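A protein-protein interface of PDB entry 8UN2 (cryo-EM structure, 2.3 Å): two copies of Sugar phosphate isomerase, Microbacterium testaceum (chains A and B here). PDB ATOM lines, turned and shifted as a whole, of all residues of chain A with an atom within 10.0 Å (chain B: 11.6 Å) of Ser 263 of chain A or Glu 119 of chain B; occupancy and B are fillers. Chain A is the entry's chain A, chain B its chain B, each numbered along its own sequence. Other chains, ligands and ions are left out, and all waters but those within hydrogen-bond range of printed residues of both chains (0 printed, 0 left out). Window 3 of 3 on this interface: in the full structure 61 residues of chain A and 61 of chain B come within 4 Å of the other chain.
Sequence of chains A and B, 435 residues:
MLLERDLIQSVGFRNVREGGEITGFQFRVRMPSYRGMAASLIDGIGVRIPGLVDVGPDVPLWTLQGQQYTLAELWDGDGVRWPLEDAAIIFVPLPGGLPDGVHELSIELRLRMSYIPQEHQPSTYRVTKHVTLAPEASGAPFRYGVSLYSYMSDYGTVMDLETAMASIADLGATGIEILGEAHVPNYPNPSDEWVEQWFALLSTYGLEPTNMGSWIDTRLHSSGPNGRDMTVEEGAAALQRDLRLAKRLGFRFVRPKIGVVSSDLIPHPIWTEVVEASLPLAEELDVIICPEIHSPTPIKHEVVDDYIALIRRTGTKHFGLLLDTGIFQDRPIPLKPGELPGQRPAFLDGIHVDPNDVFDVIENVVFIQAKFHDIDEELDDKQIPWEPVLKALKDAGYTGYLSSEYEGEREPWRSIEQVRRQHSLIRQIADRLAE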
ATOM      1  N   ARG A 219     -25.720 -34.090 -29.026  1.00  0.00           N
ATOM      2  CA  ARG A 219     -26.694 -34.489 -28.022  1.00  0.00           C
ATOM      3  C   ARG A 219     -27.951 -35.047 -28.662  1.00  0.00           C
ATOM      4  O   ARG A 219     -29.059 -34.789 -28.189  1.00  0.00           O
ATOM      5  CB  ARG A 219     -27.034 -33.317 -27.107  1.00  0.00           C
ATOM      6  CG  ARG A 219     -25.871 -32.842 -26.285  1.00  0.00           C
ATOM      7  CD  ARG A 219     -26.229 -31.615 -25.501  1.00  0.00           C
ATOM      8  NE  ARG A 219     -25.067 -30.773 -25.274  1.00  0.00           N
ATOM      9  CZ  ARG A 219     -25.128 -29.462 -25.094  1.00  0.00           C
ATOM     10  NH1 ARG A 219     -26.297 -28.847 -25.113  1.00  0.00           N
ATOM     11  NH2 ARG A 219     -24.022 -28.769 -24.896  1.00  0.00           N
ATOM     12  N   GLY A 259     -21.435 -29.718 -31.776  1.00  0.00           N
ATOM     13  CA  GLY A 259     -21.853 -29.455 -30.420  1.00  0.00           C
ATOM     14  C   GLY A 259     -20.687 -29.241 -29.476  1.00  0.00           C
ATOM     15  O   GLY A 259     -19.560 -29.648 -29.729  1.00  0.00           O
ATOM     16  N   VAL A 260     -20.978 -28.593 -28.354  1.00  0.00           N
ATOM     17  CA  VAL A 260     -19.957 -28.173 -27.406  1.00  0.00           C
ATOM     18  C   VAL A 260     -20.077 -28.992 -26.131  1.00  0.00           C
ATOM     19  O   VAL A 260     -21.102 -29.621 -25.859  1.00  0.00           O
ATOM     20  CB  VAL A 260     -20.060 -26.669 -27.102  1.00  0.00           C
ATOM     21  CG1 VAL A 260     -19.863 -25.880 -28.365  1.00  0.00           C
ATOM     22  CG2 VAL A 260     -21.402 -26.352 -26.494  1.00  0.00           C
ATOM     23  N   VAL A 261     -19.000 -28.995 -25.347  1.00  0.00           N
ATOM     24  CA  VAL A 261     -18.919 -29.773 -24.119  1.00  0.00           C
ATOM     25  C   VAL A 261     -18.565 -28.916 -22.911  1.00  0.00           C
ATOM     26  O   VAL A 261     -18.376 -29.448 -21.820  1.00  0.00           O
ATOM     27  CB  VAL A 261     -17.918 -30.937 -24.249  1.00  0.00           C
ATOM     28  CG1 VAL A 261     -18.324 -31.892 -25.336  1.00  0.00           C
ATOM     29  CG2 VAL A 261     -16.532 -30.400 -24.515  1.00  0.00           C
ATOM     30  N   SER A 262     -18.467 -27.602 -23.076  1.00  0.00           N
ATOM     31  CA  SER A 262     -18.058 -26.749 -21.969  1.00  0.00           C
ATOM     32  C   SER A 262     -18.648 -25.364 -22.162  1.00  0.00           C
ATOM     33  O   SER A 262     -19.283 -25.071 -23.174  1.00  0.00           O
ATOM     34  CB  SER A 262     -16.537 -26.664 -21.863  1.00  0.00           C
ATOM     35  OG  SER A 262     -16.029 -25.740 -22.806  1.00  0.00           O
ATOM     36  N   SER A 263     -18.412 -24.505 -21.170  1.00  0.00           N
ATOM     37  CA  SER A 263     -18.932 -23.146 -21.215  1.00  0.00           C
ATOM     38  C   SER A 263     -18.151 -22.254 -22.167  1.00  0.00           C
ATOM     39  O   SER A 263     -18.671 -21.220 -22.595  1.00  0.00           O
ATOM     40  CB  SER A 263     -18.921 -22.535 -19.817  1.00  0.00           C
ATOM     41  OG  SER A 263     -17.612 -22.143 -19.447  1.00  0.00           O
ATOM     42  N   ASP A 264     -16.922 -22.627 -22.514  1.00  0.00           N
ATOM     43  CA  ASP A 264     -16.085 -21.832 -23.398  1.00  0.00           C
ATOM     44  C   ASP A 264     -16.304 -22.166 -24.864  1.00  0.00           C
ATOM     45  O   ASP A 264     -15.488 -21.771 -25.703  1.00  0.00           O
ATOM     46  CB  ASP A 264     -14.615 -22.024 -23.036  1.00  0.00           C
ATOM     47  CG  ASP A 264     -14.266 -21.421 -21.697  1.00  0.00           C
ATOM     48  OD1 ASP A 264     -14.897 -20.412 -21.318  1.00  0.00           O
ATOM     49  OD2 ASP A 264     -13.367 -21.957 -21.018  1.00  0.00           O
ATOM     50  N   LEU A 265     -17.393 -22.883 -25.172  1.00  0.00           N
ATOM     51  CA  LEU A 265     -17.721 -23.397 -26.507  1.00  0.00           C
ATOM     52  C   LEU A 265     -16.587 -24.245 -27.075  1.00  0.00           C
ATOM     53  O   LEU A 265     -16.274 -24.181 -28.263  1.00  0.00           O
ATOM     54  CB  LEU A 265     -18.101 -22.274 -27.475  1.00  0.00           C
ATOM     55  CG  LEU A 265     -19.215 -21.314 -27.066  1.00  0.00           C
ATOM     56  CD1 LEU A 265     -19.625 -20.495 -28.267  1.00  0.00           C
ATOM     57  CD2 LEU A 265     -20.407 -22.050 -26.499  1.00  0.00           C
ATOM     58  N   ILE A 266     -15.958 -25.029 -26.207  1.00  0.00           N
ATOM     59  CA  ILE A 266     -14.976 -26.011 -26.671  1.00  0.00           C
ATOM     60  C   ILE A 266     -15.710 -27.094 -27.440  1.00  0.00           C
ATOM     61  O   ILE A 266     -16.714 -27.629 -26.934  1.00  0.00           O
ATOM     62  CB  ILE A 266     -14.210 -26.605 -25.478  1.00  0.00           C
ATOM     63  CG1 ILE A 266     -13.290 -25.554 -24.862  1.00  0.00           C
ATOM     64  CG2 ILE A 266     -13.413 -27.823 -25.895  1.00  0.00           C
ATOM     65  CD1 ILE A 266     -12.346 -24.909 -25.849  1.00  0.00           C
ATOM     66  N   PRO A 267     -15.292 -27.429 -28.660  1.00  0.00           N
ATOM     67  CA  PRO A 267     -16.031 -28.414 -29.454  1.00  0.00           C
ATOM     68  C   PRO A 267     -15.956 -29.808 -28.857  1.00  0.00           C
ATOM     69  O   PRO A 267     -15.098 -30.106 -28.025  1.00  0.00           O
ATOM     70  CB  PRO A 267     -15.334 -28.361 -30.817  1.00  0.00           C
ATOM     71  CG  PRO A 267     -14.615 -27.073 -30.833  1.00  0.00           C
ATOM     72  CD  PRO A 267     -14.205 -26.811 -29.430  1.00  0.00           C
ATOM     73  N   SER A 295     -18.782 -14.987 -32.336  1.00  0.00           N
ATOM     74  CA  SER A 295     -18.705 -14.519 -30.960  1.00  0.00           C
ATOM     75  C   SER A 295     -19.448 -15.478 -30.036  1.00  0.00           C
ATOM     76  O   SER A 295     -20.502 -16.000 -30.418  1.00  0.00           O
ATOM     77  CB  SER A 295     -19.309 -13.121 -30.881  1.00  0.00           C
ATOM     78  OG  SER A 295     -19.292 -12.601 -29.571  1.00  0.00           O
ATOM     79  N   PRO A 296     -18.952 -15.734 -28.817  1.00  0.00           N
ATOM     80  CA  PRO A 296     -17.853 -15.126 -28.067  1.00  0.00           C
ATOM     81  C   PRO A 296     -16.458 -15.647 -28.348  1.00  0.00           C
ATOM     82  O   PRO A 296     -15.585 -15.397 -27.529  1.00  0.00           O
ATOM     83  CB  PRO A 296     -18.223 -15.453 -26.628  1.00  0.00           C
ATOM     84  CG  PRO A 296     -18.853 -16.763 -26.731  1.00  0.00           C
ATOM     85  CD  PRO A 296     -19.644 -16.745 -28.004  1.00  0.00           C
ATOM     86  N   THR A 297     -16.238 -16.353 -29.444  1.00  0.00           N
ATOM     87  CA  THR A 297     -14.893 -16.811 -29.767  1.00  0.00           C
ATOM     88  C   THR A 297     -14.161 -15.740 -30.565  1.00  0.00           C
ATOM     89  O   THR A 297     -14.594 -15.410 -31.673  1.00  0.00           O
ATOM     90  CB  THR A 297     -14.936 -18.104 -30.563  1.00  0.00           C
ATOM     91  OG1 THR A 297     -15.649 -19.097 -29.823  1.00  0.00           O
ATOM     92  CG2 THR A 297     -13.539 -18.596 -30.846  1.00  0.00           C
ATOM     93  N   HIS A 301      -7.721 -17.368 -30.443  1.00  0.00           N
ATOM     94  CA  HIS A 301      -8.323 -18.362 -29.570  1.00  0.00           C
ATOM     95  C   HIS A 301      -7.728 -19.729 -29.863  1.00  0.00           C
ATOM     96  O   HIS A 301      -7.170 -19.971 -30.933  1.00  0.00           O
ATOM     97  CB  HIS A 301      -9.845 -18.396 -29.730  1.00  0.00           C
ATOM     98  CG  HIS A 301     -10.561 -19.000 -28.567  1.00  0.00           C
ATOM     99  ND1 HIS A 301     -10.907 -20.332 -28.519  1.00  0.00           N
ATOM    100  CD2 HIS A 301     -10.990 -18.458 -27.404  1.00  0.00           C
ATOM    101  CE1 HIS A 301     -11.525 -20.583 -27.379  1.00  0.00           C
ATOM    102  NE2 HIS A 301     -11.587 -19.462 -26.684  1.00  0.00           N
ATOM    103  N   VAL A 303      -9.403 -22.535 -30.081  1.00  0.00           N
ATOM    104  CA  VAL A 303     -10.264 -23.258 -31.010  1.00  0.00           C
ATOM    105  C   VAL A 303      -9.891 -22.919 -32.445  1.00  0.00           C
ATOM    106  O   VAL A 303      -9.820 -23.799 -33.312  1.00  0.00           O
ATOM    107  CB  VAL A 303     -11.739 -22.935 -30.702  1.00  0.00           C
ATOM    108  CG1 VAL A 303     -12.661 -23.366 -31.824  1.00  0.00           C
ATOM    109  CG2 VAL A 303     -12.151 -23.587 -29.404  1.00  0.00           C
ATOM    110  N   PRO A 345     -25.886 -13.008 -21.156  1.00  0.00           N
ATOM    111  CA  PRO A 345     -24.432 -13.201 -21.165  1.00  0.00           C
ATOM    112  C   PRO A 345     -23.692 -11.952 -21.614  1.00  0.00           C
ATOM    113  O   PRO A 345     -24.232 -11.098 -22.317  1.00  0.00           O
ATOM    114  CB  PRO A 345     -24.234 -14.354 -22.151  1.00  0.00           C
ATOM    115  CG  PRO A 345     -25.533 -15.059 -22.176  1.00  0.00           C
ATOM    116  CD  PRO A 345     -26.568 -14.003 -22.000  1.00  0.00           C
ATOM    117  N   PHE A 347     -21.205 -11.435 -23.596  1.00  0.00           N
ATOM    118  CA  PHE A 347     -20.725 -11.265 -24.958  1.00  0.00           C
ATOM    119  C   PHE A 347     -21.753 -10.605 -25.860  1.00  0.00           C
ATOM    120  O   PHE A 347     -21.450 -10.338 -27.025  1.00  0.00           O
ATOM    121  CB  PHE A 347     -20.281 -12.607 -25.544  1.00  0.00           C
ATOM    122  CG  PHE A 347     -21.408 -13.501 -25.975  1.00  0.00           C
ATOM    123  CD1 PHE A 347     -21.771 -13.596 -27.311  1.00  0.00           C
ATOM    124  CD2 PHE A 347     -22.075 -14.283 -25.053  1.00  0.00           C
ATOM    125  CE1 PHE A 347     -22.798 -14.420 -27.707  1.00  0.00           C
ATOM    126  CE2 PHE A 347     -23.099 -15.118 -25.447  1.00  0.00           C
ATOM    127  CZ  PHE A 347     -23.461 -15.184 -26.774  1.00  0.00           C
ATOM    128  N   LEU B 111     -36.438 -27.652 -26.324  1.00  0.00           N
ATOM    129  CA  LEU B 111     -35.642 -28.218 -27.397  1.00  0.00           C
ATOM    130  C   LEU B 111     -34.191 -28.252 -26.962  1.00  0.00           C
ATOM    131  O   LEU B 111     -33.731 -27.362 -26.249  1.00  0.00           O
ATOM    132  CB  LEU B 111     -35.764 -27.404 -28.678  1.00  0.00           C
ATOM    133  CG  LEU B 111     -37.155 -27.203 -29.258  1.00  0.00           C
ATOM    134  CD1 LEU B 111     -37.095 -26.226 -30.398  1.00  0.00           C
ATOM    135  CD2 LEU B 111     -37.713 -28.520 -29.722  1.00  0.00           C
ATOM    136  N   ARG B 112     -33.469 -29.276 -27.393  1.00  0.00           N
ATOM    137  CA  ARG B 112     -32.053 -29.407 -27.081  1.00  0.00           C
ATOM    138  C   ARG B 112     -31.226 -28.932 -28.266  1.00  0.00           C
ATOM    139  O   ARG B 112     -31.290 -29.518 -29.347  1.00  0.00           O
ATOM    140  CB  ARG B 112     -31.700 -30.848 -26.727  1.00  0.00           C
ATOM    141  CG  ARG B 112     -32.446 -31.377 -25.538  1.00  0.00           C
ATOM    142  CD  ARG B 112     -31.760 -32.583 -24.946  1.00  0.00           C
ATOM    143  NE  ARG B 112     -31.410 -33.571 -25.953  1.00  0.00           N
ATOM    144  CZ  ARG B 112     -32.242 -34.490 -26.419  1.00  0.00           C
ATOM    145  NH1 ARG B 112     -33.483 -34.550 -25.976  1.00  0.00           N
ATOM    146  NH2 ARG B 112     -31.835 -35.349 -27.332  1.00  0.00           N
ATOM    147  N   MET B 113     -30.462 -27.868 -28.060  1.00  0.00           N
ATOM    148  CA  MET B 113     -29.481 -27.396 -29.022  1.00  0.00           C
ATOM    149  C   MET B 113     -28.113 -27.846 -28.539  1.00  0.00           C
ATOM    150  O   MET B 113     -27.740 -27.574 -27.397  1.00  0.00           O
ATOM    151  CB  MET B 113     -29.529 -25.878 -29.151  1.00  0.00           C
ATOM    152  CG  MET B 113     -30.914 -25.285 -29.104  1.00  0.00           C
ATOM    153  SD  MET B 113     -31.924 -25.746 -30.508  1.00  0.00           S
ATOM    154  CE  MET B 113     -33.413 -24.834 -30.147  1.00  0.00           C
ATOM    155  N   SER B 114     -27.370 -28.538 -29.397  1.00  0.00           N
ATOM    156  CA  SER B 114     -26.117 -29.132 -28.954  1.00  0.00           C
ATOM    157  C   SER B 114     -24.981 -28.124 -28.883  1.00  0.00           C
ATOM    158  O   SER B 114     -24.002 -28.367 -28.175  1.00  0.00           O
ATOM    159  CB  SER B 114     -25.731 -30.280 -29.876  1.00  0.00           C
ATOM    160  OG  SER B 114     -26.855 -31.091 -30.147  1.00  0.00           O
ATOM    161  N   TYR B 115     -25.091 -27.003 -29.575  1.00  0.00           N
ATOM    162  CA  TYR B 115     -24.034 -26.008 -29.634  1.00  0.00           C
ATOM    163  C   TYR B 115     -24.109 -24.999 -28.502  1.00  0.00           C
ATOM    164  O   TYR B 115     -23.304 -24.066 -28.468  1.00  0.00           O
ATOM    165  CB  TYR B 115     -24.076 -25.283 -30.983  1.00  0.00           C
ATOM    166  CG  TYR B 115     -25.460 -24.870 -31.418  1.00  0.00           C
ATOM    167  CD1 TYR B 115     -26.002 -23.669 -31.004  1.00  0.00           C
ATOM    168  CD2 TYR B 115     -26.218 -25.679 -32.251  1.00  0.00           C
ATOM    169  CE1 TYR B 115     -27.254 -23.289 -31.391  1.00  0.00           C
ATOM    170  CE2 TYR B 115     -27.475 -25.310 -32.637  1.00  0.00           C
ATOM    171  CZ  TYR B 115     -27.986 -24.115 -32.203  1.00  0.00           C
ATOM    172  OH  TYR B 115     -29.242 -23.731 -32.598  1.00  0.00           O
ATOM    173  N   ILE B 116     -25.054 -25.158 -27.586  1.00  0.00           N
ATOM    174  CA  ILE B 116     -25.238 -24.267 -26.446  1.00  0.00           C
ATOM    175  C   ILE B 116     -24.706 -25.011 -25.228  1.00  0.00           C
ATOM    176  O   ILE B 116     -24.869 -26.237 -25.160  1.00  0.00           O
ATOM    177  CB  ILE B 116     -26.718 -23.869 -26.316  1.00  0.00           C
ATOM    178  CG1 ILE B 116     -27.126 -23.023 -27.518  1.00  0.00           C
ATOM    179  CG2 ILE B 116     -27.010 -23.114 -25.036  1.00  0.00           C
ATOM    180  CD1 ILE B 116     -28.566 -22.616 -27.513  1.00  0.00           C
ATOM    181  N   PRO B 117     -24.012 -24.346 -24.295  1.00  0.00           N
ATOM    182  CA  PRO B 117     -23.512 -25.038 -23.102  1.00  0.00           C
ATOM    183  C   PRO B 117     -24.626 -25.616 -22.246  1.00  0.00           C
ATOM    184  O   PRO B 117     -25.765 -25.154 -22.280  1.00  0.00           O
ATOM    185  CB  PRO B 117     -22.758 -23.939 -22.353  1.00  0.00           C
ATOM    186  CG  PRO B 117     -22.332 -23.017 -23.399  1.00  0.00           C
ATOM    187  CD  PRO B 117     -23.414 -23.008 -24.428  1.00  0.00           C
ATOM    188  N   GLN B 118     -24.265 -26.630 -21.458  1.00  0.00           N
ATOM    189  CA  GLN B 118     -25.247 -27.475 -20.790  1.00  0.00           C
ATOM    190  C   GLN B 118     -25.994 -26.747 -19.679  1.00  0.00           C
ATOM    191  O   GLN B 118     -27.111 -27.139 -19.327  1.00  0.00           O
ATOM    192  CB  GLN B 118     -24.543 -28.709 -20.233  1.00  0.00           C
ATOM    193  CG  GLN B 118     -25.445 -29.869 -19.904  1.00  0.00           C
ATOM    194  CD  GLN B 118     -25.884 -30.622 -21.127  1.00  0.00           C
ATOM    195  OE1 GLN B 118     -25.086 -31.303 -21.768  1.00  0.00           O
ATOM    196  NE2 GLN B 118     -27.163 -30.513 -21.460  1.00  0.00           N
ATOM    197  N   GLU B 119     -25.412 -25.685 -19.126  1.00  0.00           N
ATOM    198  CA  GLU B 119     -26.060 -24.988 -18.018  1.00  0.00           C
ATOM    199  C   GLU B 119     -27.248 -24.162 -18.494  1.00  0.00           C
ATOM    200  O   GLU B 119     -28.196 -23.932 -17.737  1.00  0.00           O
ATOM    201  CB  GLU B 119     -25.052 -24.102 -17.292  1.00  0.00           C
ATOM    202  CG  GLU B 119     -24.262 -23.187 -18.202  1.00  0.00           C
ATOM    203  CD  GLU B 119     -22.907 -23.752 -18.564  1.00  0.00           C
ATOM    204  OE1 GLU B 119     -22.837 -24.935 -18.958  1.00  0.00           O
ATOM    205  OE2 GLU B 119     -21.910 -23.012 -18.456  1.00  0.00           O
ATOM    206  N   HIS B 120     -27.220 -23.711 -19.741  1.00  0.00           N
ATOM    207  CA  HIS B 120     -28.316 -22.947 -20.312  1.00  0.00           C
ATOM    208  C   HIS B 120     -29.286 -23.811 -21.097  1.00  0.00           C
ATOM    209  O   HIS B 120     -30.005 -23.290 -21.952  1.00  0.00           O
ATOM    210  CB  HIS B 120     -27.770 -21.844 -21.212  1.00  0.00           C
ATOM    211  CG  HIS B 120     -26.895 -20.867 -20.499  1.00  0.00           C
ATOM    212  ND1 HIS B 120     -25.762 -20.328 -21.069  1.00  0.00           N
ATOM    213  CD2 HIS B 120     -26.983 -20.333 -19.259  1.00  0.00           C
ATOM    214  CE1 HIS B 120     -25.193 -19.501 -20.212  1.00  0.00           C
ATOM    215  NE2 HIS B 120     -25.914 -19.485 -19.105  1.00  0.00           N
ATOM    216  N   GLN B 121     -29.326 -25.101 -20.827  1.00  0.00           N
ATOM    217  CA  GLN B 121     -30.067 -26.056 -21.623  1.00  0.00           C
ATOM    218  C   GLN B 121     -31.080 -26.803 -20.769  1.00  0.00           C
ATOM    219  O   GLN B 121     -30.849 -27.033 -19.580  1.00  0.00           O
ATOM    220  CB  GLN B 121     -29.096 -27.044 -22.275  1.00  0.00           C
ATOM    221  CG  GLN B 121     -28.475 -26.514 -23.537  1.00  0.00           C
ATOM    222  CD  GLN B 121     -29.487 -26.259 -24.615  1.00  0.00           C
ATOM    223  OE1 GLN B 121     -29.719 -25.122 -25.013  1.00  0.00           O
ATOM    224  NE2 GLN B 121     -30.097 -27.320 -25.102  1.00  0.00           N
ATOM    225  N   PRO B 122     -32.229 -27.204 -21.339  1.00  0.00           N
ATOM    226  CA  PRO B 122     -32.701 -27.047 -22.716  1.00  0.00           C
ATOM    227  C   PRO B 122     -33.254 -25.669 -23.010  1.00  0.00           C
ATOM    228  O   PRO B 122     -33.579 -24.932 -22.091  1.00  0.00           O
ATOM    229  CB  PRO B 122     -33.800 -28.095 -22.817  1.00  0.00           C
ATOM    230  CG  PRO B 122     -34.321 -28.191 -21.469  1.00  0.00           C
ATOM    231  CD  PRO B 122     -33.161 -28.021 -20.551  1.00  0.00           C
ATOM    232  N   SER B 123     -33.318 -25.328 -24.292  1.00  0.00           N
ATOM    233  CA  SER B 123     -33.927 -24.076 -24.707  1.00  0.00           C
ATOM    234  C   SER B 123     -35.422 -24.131 -24.460  1.00  0.00           C
ATOM    235  O   SER B 123     -36.102 -25.050 -24.912  1.00  0.00           O
ATOM    236  CB  SER B 123     -33.649 -23.823 -26.182  1.00  0.00           C
ATOM    237  OG  SER B 123     -32.275 -23.597 -26.406  1.00  0.00           O
ATOM    238  N   THR B 124     -35.939 -23.146 -23.742  1.00  0.00           N
ATOM    239  CA  THR B 124     -37.329 -23.129 -23.322  1.00  0.00           C
ATOM    240  C   THR B 124     -38.049 -21.994 -24.030  1.00  0.00           C
ATOM    241  O   THR B 124     -37.530 -20.878 -24.104  1.00  0.00           O
ATOM    242  CB  THR B 124     -37.433 -22.973 -21.806  1.00  0.00           C
ATOM    243  OG1 THR B 124     -36.587 -23.936 -21.174  1.00  0.00           O
ATOM    244  CG2 THR B 124     -38.839 -23.212 -21.348  1.00  0.00           C
ATOM    245  N   ARG B 126     -41.768 -20.219 -23.922  1.00  0.00           N
ATOM    246  CA  ARG B 126     -43.060 -20.077 -23.269  1.00  0.00           C
ATOM    247  C   ARG B 126     -43.871 -19.032 -24.009  1.00  0.00           C
ATOM    248  O   ARG B 126     -43.515 -17.851 -24.001  1.00  0.00           O
ATOM    249  CB  ARG B 126     -42.900 -19.670 -21.809  1.00  0.00           C
ATOM    250  CG  ARG B 126     -42.138 -20.646 -20.978  1.00  0.00           C
ATOM    251  CD  ARG B 126     -41.892 -20.080 -19.610  1.00  0.00           C
ATOM    252  NE  ARG B 126     -40.615 -20.536 -19.084  1.00  0.00           N
ATOM    253  CZ  ARG B 126     -40.480 -21.562 -18.256  1.00  0.00           C
ATOM    254  NH1 ARG B 126     -41.550 -22.235 -17.856  1.00  0.00           N
ATOM    255  NH2 ARG B 126     -39.278 -21.915 -17.829  1.00  0.00           N
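OG of Ser 262 of chain A sits close to N of Ile 266 of chain A (3.5 Å).
NE2 of Gln 121 of chain B lies close to N of Met 113 of chain B (3.0 Å).
The guanidinium group (NH2) of Arg 219 of chain A is in hydrogen-bond range of the backbone carbonyl oxygen (O) of Val 260 of chain A (3.2 Å).
The backbone NH of Asp 264 of chain A lies within hydrogen-bond range of the side-chain hydroxyl of Ser 262 of chain A.
The side-chain hydroxyl (OG) of Ser 123 of chain B sits at hydrogen-bond distance from the side-chain amide oxygen (OE1) of Gln 121 of chain B (3.3 Å).
Hydrophobic or aromatic side chains of chain B within 4 Å of the printed part of chain A: Pro 117.
Hydrophobic or aromatic side chains of chain A that line the printed part of chain B: Val 260 and Leu 265.
Among the printed residues, no Asp or Glu carboxylate lies within 4 Å of a Lys or Arg side-chain nitrogen of the other chain.
NH2 of Arg 219 of chain A lies within hydrogen-bond range of O of Ile 116 of chain B (2.7 Å).
NH2 of Arg 112 of chain B lies within hydrogen-bond range of O of Arg 219 of chain A (3.0 Å).
O of Ser 114 of chain B lies within hydrogen-bond range of N of Val 260 of chain A (3.0 Å).
NH2 of Arg 219 of chain A lies within hydrogen-bond range of O of Ser 114 of chain B (3.3 Å).
O of Met 113 of chain B lies within hydrogen-bond range of NH1 of Arg 219 of chain A (3.0 Å).
Of chain B, only Glu 119 (3.3 Å) comes within 4 Å of Ser 263 of chain A.
Glu 119 of chain B touches just one residue of chain A: Ser 263.
No residue of chain B comes within 4 Å of Asp 264 of chain A.
Of chain B, only Pro 117 comes within 4 Å of Leu 265 of chain A.
Pro 117 of chain B touches just these residues of chain A: Val 260, Ser 262 and Leu 265.
No residue of chain A comes within 4 Å of His 120 of chain B.
Printed residues of chain A within 4 Å of Gln 121 of chain B: Arg 219 (3.6 Å).
Of the printed residues of chain A, Ile 116 of chain B touches Arg 219 and Val 260.
Of the printed residues of chain A, Gln 118 of chain B touches Arg 219.
Pro 296 of chain A touches none of the printed residues of chain B.
The nearest residue of chain B that does not touch Ser 263 of chain A is Pro 117 of chain B (4.04 Å).
The nearest residue of chain A that does not touch Glu 119 of chain B is Ser 262 of chain A (5.3 Å).
The nearest printed residue of chain A that does not touch Arg 112 of chain B is Gly 259 of chain A (9.5 Å).
Among the printed residues, pairs that only touch across the chains: Gly 259 of chain A with Ser 114 of chain B, Ser 263 of chain A with Glu 119 of chain B, Arg 219 of chain A with Gln 118 of chain B, Arg 219 of chain A with Gln 121 of chain B, Val 260 of chain A with Tyr 115 of chain B, Ser 262 of chain A with Pro 117 of chain B, Val 260 of chain A with Ile 116 of chain B, Leu 265 of chain A with Pro 117 of chain B and Val 260 of chain A with Pro 117 of chain B.
No position is printed for both chains.
Of the 14 pairs that touch across the chains among the printed residues, none has its exchanged pair printed and touching as well.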
